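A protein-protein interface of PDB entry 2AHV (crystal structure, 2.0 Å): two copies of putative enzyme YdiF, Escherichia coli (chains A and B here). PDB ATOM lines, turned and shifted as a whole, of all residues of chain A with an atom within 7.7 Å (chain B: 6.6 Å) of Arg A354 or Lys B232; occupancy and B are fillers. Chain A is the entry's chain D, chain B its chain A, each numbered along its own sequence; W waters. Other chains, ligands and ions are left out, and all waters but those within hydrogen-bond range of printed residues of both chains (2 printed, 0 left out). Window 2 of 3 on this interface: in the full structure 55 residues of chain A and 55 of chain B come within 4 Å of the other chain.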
ATOM      1  N   ALA A 325      12.187  10.437  17.830  1.00  0.00           N
ATOM      2  CA  ALA A 325      12.189   9.606  16.633  1.00  0.00           C
ATOM      3  C   ALA A 325      10.986   9.847  15.715  1.00  0.00           C
ATOM      4  O   ALA A 325      11.061   9.581  14.503  1.00  0.00           O
ATOM      5  CB  ALA A 325      12.308   8.132  17.006  1.00  0.00           C
ATOM      6  N   ASP A 326       9.889  10.363  16.268  1.00  0.00           N
ATOM      7  CA  ASP A 326       8.729  10.703  15.450  1.00  0.00           C
ATOM      8  C   ASP A 326       8.759  12.121  14.891  1.00  0.00           C
ATOM      9  O   ASP A 326       7.821  12.512  14.204  1.00  0.00           O
ATOM     10  CB  ASP A 326       7.422  10.487  16.219  1.00  0.00           C
ATOM     11  CG  ASP A 326       7.252   9.064  16.698  1.00  0.00           C
ATOM     12  OD1 ASP A 326       7.696   8.111  16.004  1.00  0.00           O
ATOM     13  OD2 ASP A 326       6.682   8.805  17.779  1.00  0.00           O
ATOM     14  N   ASP A 327       9.818  12.889  15.175  1.00  0.00           N
ATOM     15  CA  ASP A 327       9.870  14.300  14.757  1.00  0.00           C
ATOM     16  C   ASP A 327      10.731  14.569  13.526  1.00  0.00           C
ATOM     17  O   ASP A 327      10.932  15.723  13.145  1.00  0.00           O
ATOM     18  CB  ASP A 327      10.296  15.210  15.915  1.00  0.00           C
ATOM     19  CG  ASP A 327       9.415  15.034  17.146  1.00  0.00           C
ATOM     20  OD1 ASP A 327       8.192  14.829  16.992  1.00  0.00           O
ATOM     21  OD2 ASP A 327       9.864  15.075  18.311  1.00  0.00           O
ATOM     22  N   PHE A 328      11.251  13.500  12.930  1.00  0.00           N
ATOM     23  CA  PHE A 328      11.913  13.557  11.625  1.00  0.00           C
ATOM     24  C   PHE A 328      11.705  12.199  10.935  1.00  0.00           C
ATOM     25  O   PHE A 328      11.136  11.275  11.526  1.00  0.00           O
ATOM     26  CB  PHE A 328      13.407  13.907  11.752  1.00  0.00           C
ATOM     27  CG  PHE A 328      14.207  12.909  12.551  1.00  0.00           C
ATOM     28  CD1 PHE A 328      14.948  11.922  11.914  1.00  0.00           C
ATOM     29  CD2 PHE A 328      14.216  12.960  13.949  1.00  0.00           C
ATOM     30  CE1 PHE A 328      15.675  10.995  12.640  1.00  0.00           C
ATOM     31  CE2 PHE A 328      14.946  12.047  14.686  1.00  0.00           C
ATOM     32  CZ  PHE A 328      15.686  11.059  14.029  1.00  0.00           C
ATOM     33  N   ILE A 329      12.150  12.088   9.690  1.00  0.00           N
ATOM     34  CA  ILE A 329      11.953  10.860   8.910  1.00  0.00           C
ATOM     35  C   ILE A 329      13.272  10.394   8.277  1.00  0.00           C
ATOM     36  O   ILE A 329      14.014  11.190   7.679  1.00  0.00           O
ATOM     37  CB  ILE A 329      10.786  11.047   7.856  1.00  0.00           C
ATOM     38  CG1 ILE A 329      10.377   9.718   7.182  1.00  0.00           C
ATOM     39  CG2 ILE A 329      11.125  12.106   6.831  1.00  0.00           C
ATOM     40  CD1 ILE A 329       9.594   8.793   8.079  1.00  0.00           C
ATOM     41  N   LEU A 330      13.565   9.108   8.445  1.00  0.00           N
ATOM     42  CA  LEU A 330      14.734   8.492   7.829  1.00  0.00           C
ATOM     43  C   LEU A 330      14.314   7.576   6.685  1.00  0.00           C
ATOM     44  O   LEU A 330      13.425   6.732   6.838  1.00  0.00           O
ATOM     45  CB  LEU A 330      15.548   7.697   8.851  1.00  0.00           C
ATOM     46  CG  LEU A 330      16.203   8.463  10.012  1.00  0.00           C
ATOM     47  CD1 LEU A 330      17.009   7.466  10.831  1.00  0.00           C
ATOM     48  CD2 LEU A 330      17.101   9.574   9.505  1.00  0.00           C
ATOM     49  N   PRO A 336      12.431   1.705   1.242  1.00  0.00           N
ATOM     50  CA  PRO A 336      11.646   1.894   2.470  1.00  0.00           C
ATOM     51  C   PRO A 336      11.803   3.269   3.114  1.00  0.00           C
ATOM     52  O   PRO A 336      12.877   3.881   3.037  1.00  0.00           O
ATOM     53  CB  PRO A 336      12.184   0.795   3.398  1.00  0.00           C
ATOM     54  CG  PRO A 336      12.649  -0.241   2.465  1.00  0.00           C
ATOM     55  CD  PRO A 336      13.328   0.539   1.360  1.00  0.00           C
ATOM     56  N   ILE A 337      10.717   3.757   3.701  1.00  0.00           N
ATOM     57  CA  ILE A 337      10.666   5.095   4.294  1.00  0.00           C
ATOM     58  C   ILE A 337      10.078   4.965   5.681  1.00  0.00           C
ATOM     59  O   ILE A 337       8.969   4.439   5.846  1.00  0.00           O
ATOM     60  CB  ILE A 337       9.829   6.039   3.391  1.00  0.00           C
ATOM     61  CG1 ILE A 337      10.559   6.266   2.061  1.00  0.00           C
ATOM     62  CG2 ILE A 337       9.534   7.376   4.088  1.00  0.00           C
ATOM     63  CD1 ILE A 337       9.711   6.889   1.001  1.00  0.00           C
ATOM     64  N   GLY A 338      10.839   5.391   6.688  1.00  0.00           N
ATOM     65  CA  GLY A 338      10.399   5.295   8.070  1.00  0.00           C
ATOM     66  C   GLY A 338      10.558   3.899   8.633  1.00  0.00           C
ATOM     67  O   GLY A 338      11.159   3.021   8.008  1.00  0.00           O
ATOM     68  N   GLY A 339      10.017   3.690   9.828  1.00  0.00           N
ATOM     69  CA  GLY A 339      10.078   2.387  10.465  1.00  0.00           C
ATOM     70  C   GLY A 339      11.106   2.281  11.574  1.00  0.00           C
ATOM     71  O   GLY A 339      11.902   3.204  11.794  1.00  0.00           O
ATOM     72  N   ILE A 340      11.078   1.138  12.262  1.00  0.00           N
ATOM     73  CA  ILE A 340      11.937   0.847  13.408  1.00  0.00           C
ATOM     74  C   ILE A 340      12.601  -0.524  13.270  1.00  0.00           C
ATOM     75  O   ILE A 340      12.104  -1.398  12.549  1.00  0.00           O
ATOM     76  CB  ILE A 340      11.134   0.892  14.756  1.00  0.00           C
ATOM     77  CG1 ILE A 340       9.959  -0.090  14.742  1.00  0.00           C
ATOM     78  CG2 ILE A 340      10.676   2.316  15.086  1.00  0.00           C
ATOM     79  CD1 ILE A 340       9.316  -0.346  16.134  1.00  0.00           C
ATOM     80  N   VAL A 351      10.415  -2.608  10.519  1.00  0.00           N
ATOM     81  CA  VAL A 351       8.978  -2.770  10.564  1.00  0.00           C
ATOM     82  C   VAL A 351       8.318  -1.408  10.814  1.00  0.00           C
ATOM     83  O   VAL A 351       9.008  -0.418  11.053  1.00  0.00           O
ATOM     84  CB  VAL A 351       8.569  -3.809  11.645  1.00  0.00           C
ATOM     85  CG1 VAL A 351       9.207  -5.171  11.349  1.00  0.00           C
ATOM     86  CG2 VAL A 351       8.951  -3.326  13.039  1.00  0.00           C
ATOM     87  N   ASN A 352       6.988  -1.362  10.769  1.00  0.00           N
ATOM     88  CA  ASN A 352       6.255  -0.113  10.912  1.00  0.00           C
ATOM     89  C   ASN A 352       6.741   0.972   9.937  1.00  0.00           C
ATOM     90  O   ASN A 352       6.773   2.148  10.295  1.00  0.00           O
ATOM     91  CB  ASN A 352       6.293   0.398  12.362  1.00  0.00           C
ATOM     92  CG  ASN A 352       5.688  -0.593  13.351  1.00  0.00           C
ATOM     93  OD1 ASN A 352       5.151  -1.633  12.962  1.00  0.00           O
ATOM     94  ND2 ASN A 352       5.765  -0.269  14.633  1.00  0.00           N
ATOM     95  N   THR A 353       7.104   0.580   8.709  1.00  0.00           N
ATOM     96  CA  THR A 353       7.462   1.565   7.683  1.00  0.00           C
ATOM     97  C   THR A 353       6.257   2.434   7.360  1.00  0.00           C
ATOM     98  O   THR A 353       5.113   2.042   7.583  1.00  0.00           O
ATOM     99  CB  THR A 353       8.015   0.901   6.384  1.00  0.00           C
ATOM    100  OG1 THR A 353       7.036   0.016   5.819  1.00  0.00           O
ATOM    101  CG2 THR A 353       9.201  -0.016   6.693  1.00  0.00           C
ATOM    102  N   ARG A 354       6.529   3.622   6.841  1.00  0.00           N
ATOM    103  CA  ARG A 354       5.499   4.562   6.461  1.00  0.00           C
ATOM    104  C   ARG A 354       5.137   4.446   4.977  1.00  0.00           C
ATOM    105  O   ARG A 354       4.011   4.741   4.576  1.00  0.00           O
ATOM    106  CB  ARG A 354       5.959   5.977   6.796  1.00  0.00           C
ATOM    107  CG  ARG A 354       6.221   6.186   8.297  1.00  0.00           C
ATOM    108  CD  ARG A 354       4.968   6.048   9.164  1.00  0.00           C
ATOM    109  NE  ARG A 354       3.948   7.011   8.759  1.00  0.00           N
ATOM    110  CZ  ARG A 354       3.947   8.290   9.124  1.00  0.00           C
ATOM    111  NH1 ARG A 354       4.902   8.758   9.920  1.00  0.00           N
ATOM    112  NH2 ARG A 354       2.993   9.103   8.694  1.00  0.00           N
ATOM    113  N   ALA A 355       6.095   4.000   4.176  1.00  0.00           N
ATOM    114  CA  ALA A 355       5.944   3.920   2.725  1.00  0.00           C
ATOM    115  C   ALA A 355       7.107   3.116   2.170  1.00  0.00           C
ATOM    116  O   ALA A 355       8.154   3.019   2.805  1.00  0.00           O
ATOM    117  CB  ALA A 355       5.945   5.325   2.104  1.00  0.00           C
ATOM    118  N   ILE A 356       6.916   2.538   0.986  1.00  0.00           N
ATOM    119  CA  ILE A 356       8.003   1.892   0.241  1.00  0.00           C
ATOM    120  C   ILE A 356       7.934   2.335  -1.214  1.00  0.00           C
ATOM    121  O   ILE A 356       6.939   2.077  -1.907  1.00  0.00           O
ATOM    122  CB  ILE A 356       7.924   0.355   0.353  1.00  0.00           C
ATOM    123  CG1 ILE A 356       7.857  -0.078   1.818  1.00  0.00           C
ATOM    124  CG2 ILE A 356       9.136  -0.321  -0.360  1.00  0.00           C
ATOM    125  CD1 ILE A 356       7.538  -1.542   1.992  1.00  0.00           C
ATOM    126  N   GLY B  11       4.100  19.000  13.153  1.00  0.00           N
ATOM    127  CA  GLY B  11       4.483  17.945  12.225  1.00  0.00           C
ATOM    128  C   GLY B  11       3.393  17.580  11.235  1.00  0.00           C
ATOM    129  O   GLY B  11       3.608  16.729  10.376  1.00  0.00           O
ATOM    130  N   ARG B  12       2.238  18.234  11.346  1.00  0.00           N
ATOM    131  CA  ARG B  12       1.103  18.008  10.449  1.00  0.00           C
ATOM    132  C   ARG B  12       1.225  18.838   9.177  1.00  0.00           C
ATOM    133  O   ARG B  12       1.635  20.001   9.231  1.00  0.00           O
ATOM    134  CB  ARG B  12      -0.212  18.381  11.135  1.00  0.00           C
ATOM    135  CG  ARG B  12      -0.564  17.545  12.354  1.00  0.00           C
ATOM    136  CD  ARG B  12      -1.854  17.992  13.030  1.00  0.00           C
ATOM    137  NE  ARG B  12      -2.265  17.001  14.018  1.00  0.00           N
ATOM    138  CZ  ARG B  12      -3.204  16.076  13.836  1.00  0.00           C
ATOM    139  NH1 ARG B  12      -3.892  16.012  12.705  1.00  0.00           N
ATOM    140  NH2 ARG B  12      -3.471  15.224  14.813  1.00  0.00           N
ATOM    141  N   ASP B 192      -2.735  10.637   5.234  1.00  0.00           N
ATOM    142  CA  ASP B 192      -2.707  10.765   6.689  1.00  0.00           C
ATOM    143  C   ASP B 192      -2.352  12.206   7.103  1.00  0.00           C
ATOM    144  O   ASP B 192      -2.216  13.081   6.237  1.00  0.00           O
ATOM    145  CB  ASP B 192      -1.848   9.668   7.359  1.00  0.00           C
ATOM    146  CG  ASP B 192      -0.349   9.898   7.237  1.00  0.00           C
ATOM    147  OD1 ASP B 192       0.100  10.939   6.717  1.00  0.00           O
ATOM    148  OD2 ASP B 192       0.465   9.054   7.667  1.00  0.00           O
ATOM    149  N   SER B 193      -2.239  12.465   8.406  1.00  0.00           N
ATOM    150  CA  SER B 193      -2.009  13.840   8.890  1.00  0.00           C
ATOM    151  C   SER B 193      -0.642  14.418   8.511  1.00  0.00           C
ATOM    152  O   SER B 193      -0.433  15.624   8.616  1.00  0.00           O
ATOM    153  CB  SER B 193      -2.188  13.907  10.407  1.00  0.00           C
ATOM    154  OG  SER B 193      -1.304  13.000  11.021  1.00  0.00           O
ATOM    155  N   GLU B 194       0.281  13.562   8.076  1.00  0.00           N
ATOM    156  CA  GLU B 194       1.593  14.016   7.599  1.00  0.00           C
ATOM    157  C   GLU B 194       1.709  14.049   6.074  1.00  0.00           C
ATOM    158  O   GLU B 194       2.791  14.294   5.538  1.00  0.00           O
ATOM    159  CB  GLU B 194       2.695  13.162   8.208  1.00  0.00           C
ATOM    160  CG  GLU B 194       2.709  13.262   9.723  1.00  0.00           C
ATOM    161  CD  GLU B 194       3.856  12.510  10.360  1.00  0.00           C
ATOM    162  OE1 GLU B 194       4.216  11.418   9.872  1.00  0.00           O
ATOM    163  OE2 GLU B 194       4.392  13.019  11.363  1.00  0.00           O
ATOM    164  N   GLY B 195       0.596  13.795   5.390  1.00  0.00           N
ATOM    165  CA  GLY B 195       0.538  13.861   3.929  1.00  0.00           C
ATOM    166  C   GLY B 195       0.816  12.579   3.151  1.00  0.00           C
ATOM    167  O   GLY B 195       0.839  12.610   1.919  1.00  0.00           O
ATOM    168  N   TYR B 196       1.047  11.459   3.840  1.00  0.00           N
ATOM    169  CA  TYR B 196       1.282  10.168   3.168  1.00  0.00           C
ATOM    170  C   TYR B 196       0.011   9.736   2.453  1.00  0.00           C
ATOM    171  O   TYR B 196      -1.032   9.609   3.087  1.00  0.00           O
ATOM    172  CB  TYR B 196       1.715   9.099   4.184  1.00  0.00           C
ATOM    173  CG  TYR B 196       3.128   9.320   4.661  1.00  0.00           C
ATOM    174  CD1 TYR B 196       4.183   8.586   4.122  1.00  0.00           C
ATOM    175  CD2 TYR B 196       3.418  10.314   5.599  1.00  0.00           C
ATOM    176  CE1 TYR B 196       5.487   8.804   4.535  1.00  0.00           C
ATOM    177  CE2 TYR B 196       4.720  10.542   6.023  1.00  0.00           C
ATOM    178  CZ  TYR B 196       5.748   9.792   5.489  1.00  0.00           C
ATOM    179  OH  TYR B 196       7.041  10.016   5.912  1.00  0.00           O
ATOM    180  N   VAL B 230      -6.736  10.804   7.296  1.00  0.00           N
ATOM    181  CA  VAL B 230      -6.843   9.784   8.345  1.00  0.00           C
ATOM    182  C   VAL B 230      -5.717   9.975   9.369  1.00  0.00           C
ATOM    183  O   VAL B 230      -4.806  10.772   9.139  1.00  0.00           O
ATOM    184  CB  VAL B 230      -6.787   8.365   7.741  1.00  0.00           C
ATOM    185  CG1 VAL B 230      -7.929   8.147   6.714  1.00  0.00           C
ATOM    186  CG2 VAL B 230      -5.430   8.102   7.098  1.00  0.00           C
ATOM    187  N   LYS B 231      -5.786   9.260  10.489  1.00  0.00           N
ATOM    188  CA  LYS B 231      -4.766   9.346  11.529  1.00  0.00           C
ATOM    189  C   LYS B 231      -3.399   8.959  10.975  1.00  0.00           C
ATOM    190  O   LYS B 231      -3.282   8.061  10.123  1.00  0.00           O
ATOM    191  CB  LYS B 231      -5.139   8.443  12.706  1.00  0.00           C
ATOM    192  CG  LYS B 231      -4.177   8.444  13.895  1.00  0.00           C
ATOM    193  CD  LYS B 231      -4.761   7.565  15.031  1.00  0.00           C
ATOM    194  CE  LYS B 231      -3.772   7.450  16.191  1.00  0.00           C
ATOM    195  NZ  LYS B 231      -4.225   6.433  17.190  1.00  0.00           N
ATOM    196  N   LYS B 232      -2.386   9.675  11.450  1.00  0.00           N
ATOM    197  CA  LYS B 232      -0.987   9.403  11.154  1.00  0.00           C
ATOM    198  C   LYS B 232      -0.659   7.916  11.217  1.00  0.00           C
ATOM    199  O   LYS B 232      -1.057   7.217  12.167  1.00  0.00           O
ATOM    200  CB  LYS B 232      -0.097  10.193  12.135  1.00  0.00           C
ATOM    201  CG  LYS B 232       1.396   9.923  12.058  1.00  0.00           C
ATOM    202  CD  LYS B 232       2.184  10.738  13.112  1.00  0.00           C
ATOM    203  CE  LYS B 232       3.570  10.119  13.353  1.00  0.00           C
ATOM    204  NZ  LYS B 232       4.793  11.046  13.250  1.00  0.00           N
ATOM    205  N   ALA B 233       0.070   7.446  10.200  1.00  0.00           N
ATOM    206  CA  ALA B 233       0.643   6.099  10.163  1.00  0.00           C
ATOM    207  C   ALA B 233      -0.379   4.964  10.309  1.00  0.00           C
ATOM    208  O   ALA B 233      -0.057   3.914  10.858  1.00  0.00           O
ATOM    209  CB  ALA B 233       1.765   5.954  11.223  1.00  0.00           C
ATOM    210  N   THR B 234      -1.607   5.167   9.829  1.00  0.00           N
ATOM    211  CA  THR B 234      -2.584   4.073   9.847  1.00  0.00           C
ATOM    212  C   THR B 234      -2.835   3.471   8.473  1.00  0.00           C
ATOM    213  O   THR B 234      -3.628   2.537   8.343  1.00  0.00           O
ATOM    214  CB  THR B 234      -3.926   4.494  10.477  1.00  0.00           C
ATOM    215  OG1 THR B 234      -4.470   5.613   9.751  1.00  0.00           O
ATOM    216  CG2 THR B 234      -3.730   4.970  11.942  1.00  0.00           C
ATOM    217  N   LEU B 235      -2.199   4.024   7.441  1.00  0.00           N
ATOM    218  CA  LEU B 235      -2.365   3.490   6.092  1.00  0.00           C
ATOM    219  C   LEU B 235      -1.321   2.405   5.855  1.00  0.00           C
ATOM    220  O   LEU B 235      -0.265   2.392   6.504  1.00  0.00           O
ATOM    221  CB  LEU B 235      -2.251   4.597   5.036  1.00  0.00           C
ATOM    222  CG  LEU B 235      -3.281   5.722   5.121  1.00  0.00           C
ATOM    223  CD1 LEU B 235      -2.854   6.922   4.264  1.00  0.00           C
ATOM    224  CD2 LEU B 235      -4.687   5.232   4.742  1.00  0.00           C
ATOM    225  N   HIS B 236      -1.621   1.486   4.941  1.00  0.00           N
ATOM    226  CA  HIS B 236      -0.687   0.401   4.622  1.00  0.00           C
ATOM    227  C   HIS B 236       0.535   0.944   3.883  1.00  0.00           C
ATOM    228  O   HIS B 236       0.381   1.543   2.828  1.00  0.00           O
ATOM    229  CB  HIS B 236      -1.383  -0.676   3.778  1.00  0.00           C
ATOM    230  CG  HIS B 236      -0.664  -1.990   3.786  1.00  0.00           C
ATOM    231  ND1 HIS B 236       0.572  -2.162   3.201  1.00  0.00           N
ATOM    232  CD2 HIS B 236      -1.004  -3.192   4.315  1.00  0.00           C
ATOM    233  CE1 HIS B 236       0.966  -3.410   3.374  1.00  0.00           C
ATOM    234  NE2 HIS B 236       0.033  -4.052   4.053  1.00  0.00           N
ATOM    235  N   PRO B 237       1.749   0.732   4.401  1.00  0.00           N
ATOM    236  CA  PRO B 237       2.942   1.305   3.758  1.00  0.00           C
ATOM    237  C   PRO B 237       3.098   0.943   2.279  1.00  0.00           C
ATOM    238  O   PRO B 237       3.605   1.756   1.521  1.00  0.00           O
ATOM    239  CB  PRO B 237       4.110   0.751   4.582  1.00  0.00           C
ATOM    240  CG  PRO B 237       3.543  -0.381   5.383  1.00  0.00           C
ATOM    241  CD  PRO B 237       2.094  -0.040   5.610  1.00  0.00           C
ATOM    242  N   LYS B 238       2.659  -0.255   1.881  1.00  0.00           N
ATOM    243  CA  LYS B 238       2.751  -0.682   0.470  1.00  0.00           C
ATOM    244  C   LYS B 238       1.673  -0.076  -0.428  1.00  0.00           C
ATOM    245  O   LYS B 238       1.754  -0.188  -1.649  1.00  0.00           O
ATOM    246  CB  LYS B 238       2.819  -2.220   0.334  1.00  0.00           C
ATOM    247  CG  LYS B 238       4.168  -2.794   0.832  1.00  0.00           C
ATOM    248  CD  LYS B 238       4.299  -4.299   0.678  1.00  0.00           C
ATOM    249  CE  LYS B 238       5.718  -4.758   0.973  1.00  0.00           C
ATOM    250  NZ  LYS B 238       5.806  -6.240   1.267  1.00  0.00           N
ATOM    251  N   VAL B 240       0.954   3.253   0.010  1.00  0.00           N
ATOM    252  CA  VAL B 240       1.303   4.676  -0.035  1.00  0.00           C
ATOM    253  C   VAL B 240       2.118   4.947  -1.302  1.00  0.00           C
ATOM    254  O   VAL B 240       3.145   4.312  -1.528  1.00  0.00           O
ATOM    255  CB  VAL B 240       2.086   5.120   1.223  1.00  0.00           C
ATOM    256  CG1 VAL B 240       2.619   6.532   1.064  1.00  0.00           C
ATOM    257  CG2 VAL B 240       1.212   4.994   2.483  1.00  0.00           C
HETATM  258  O   HOH W   1       4.011   0.669  -2.480  1.00  0.00           O
HETATM  259  O   HOH W   2       6.366   8.632  13.355  1.00  0.00           O
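Of chain B, only Asp B192, Glu B194, Tyr B196, Lys B232, Ala B233, Pro B237 and Val B240 come within 4 Å of Arg A354.
Of the printed residues of chain B, Ile A356 touches Pro B237 and Lys B238.
Of the printed residues of chain A, Asp B192 touches Arg A354 (2.7 Å).
Printed residues of chain A within 4 Å of Val B240: Arg A354 and Ala A355.
The nearest residue of chain B that does not touch Arg A354 is His B236 (5.1 Å).
The nearest residue of chain A that does not touch Lys B232 is Asp A327 (5.7 Å).
Water W1 bridges the backbone carbonyl oxygen (O) of Lys B238 (2.6 Å) and the backbone carbonyl oxygen (O) of Ile A356 (3.3 Å).
Water W2 bridges NZ of Lys B232 (2.9 Å) and OD1 of Asp A326 (3.0 Å).
No position is printed for both chains.
ND1 of His B236 sits at hydrogen-bond distance from N of Lys B238, at 3.1 Å.
N of Ile A337 lies within hydrogen-bond range of O of Ala A355 (2.8 Å).
OE2 of Glu B194 lies within salt-bridge range of NZ of Lys B232 (2.8 Å).
The backbone NH (N) of Gly B195 is in hydrogen-bond range of the side-chain carboxylate (OD1) of Asp B192, at 3.2 Å.
The backbone carbonyl oxygen (O) of Ile A337 sits at hydrogen-bond distance from the backbone NH (N) of Arg A354, at 2.8 Å.
N of Ala B233 sits at hydrogen-bond distance from OD2 of Asp B192 (3.0 Å).
Among the printed residues, pairs that only touch across the chains: Thr A353 with Pro B237 (3.3 Å), Arg A354 with Tyr B196 (3.4 Å), Ala A355 with Pro B237 (3.4 Å), Arg A354 with Ala B233 (3.5 Å), Arg A354 with Val B240 (3.5 Å), Ile A329 with Tyr B196 (3.6 Å), Ala A355 with Val B240 (3.7 Å), Arg A354 with Pro B237 (3.7 Å), Ile A356 with Lys B238 (3.8 Å) and Arg A354 with Lys B232 (3.8 Å).
Of the 17 printed residues of chain A, 6 touch a printed residue of chain B.
Printed residues of chain A that touch a printed residue of chain B: Asp A326, Ile A329, Thr A353, Arg A354, Ala A355 and Ile A356.
Of the 17 printed residues of chain B, 8 touch a printed residue of chain A.
Hydrophobic or aromatic side chains of chain B within 4 Å of the printed part of chain A: Tyr B196, Ala B233, Pro B237 and Val B240.
Along chain B the printed residues that touch a printed residue of chain A span positions 192 to 240.
Among the printed residues, 14 pairs touch across the chains.
Among the printed residues, Asp or Glu carboxylates within 4 Å of a Lys or Arg side-chain nitrogen of the other chain: Arg A354 with Asp B192 and Arg A354 with Glu B194.
The side-chain carboxylate (OD2) of Asp B192 lies within salt-bridge range of the guanidinium group (NH2) of Arg A354.
OE1 of Glu B194 is in salt-bridge range of NH1 of Arg A354 (2.7 Å).
The side-chain amino group (NZ) of Lys B232 lies within hydrogen-bond range of the backbone carbonyl oxygen (O) of Asp A326.
O of Pro B237 is in hydrogen-bond range of N of Ile A356.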
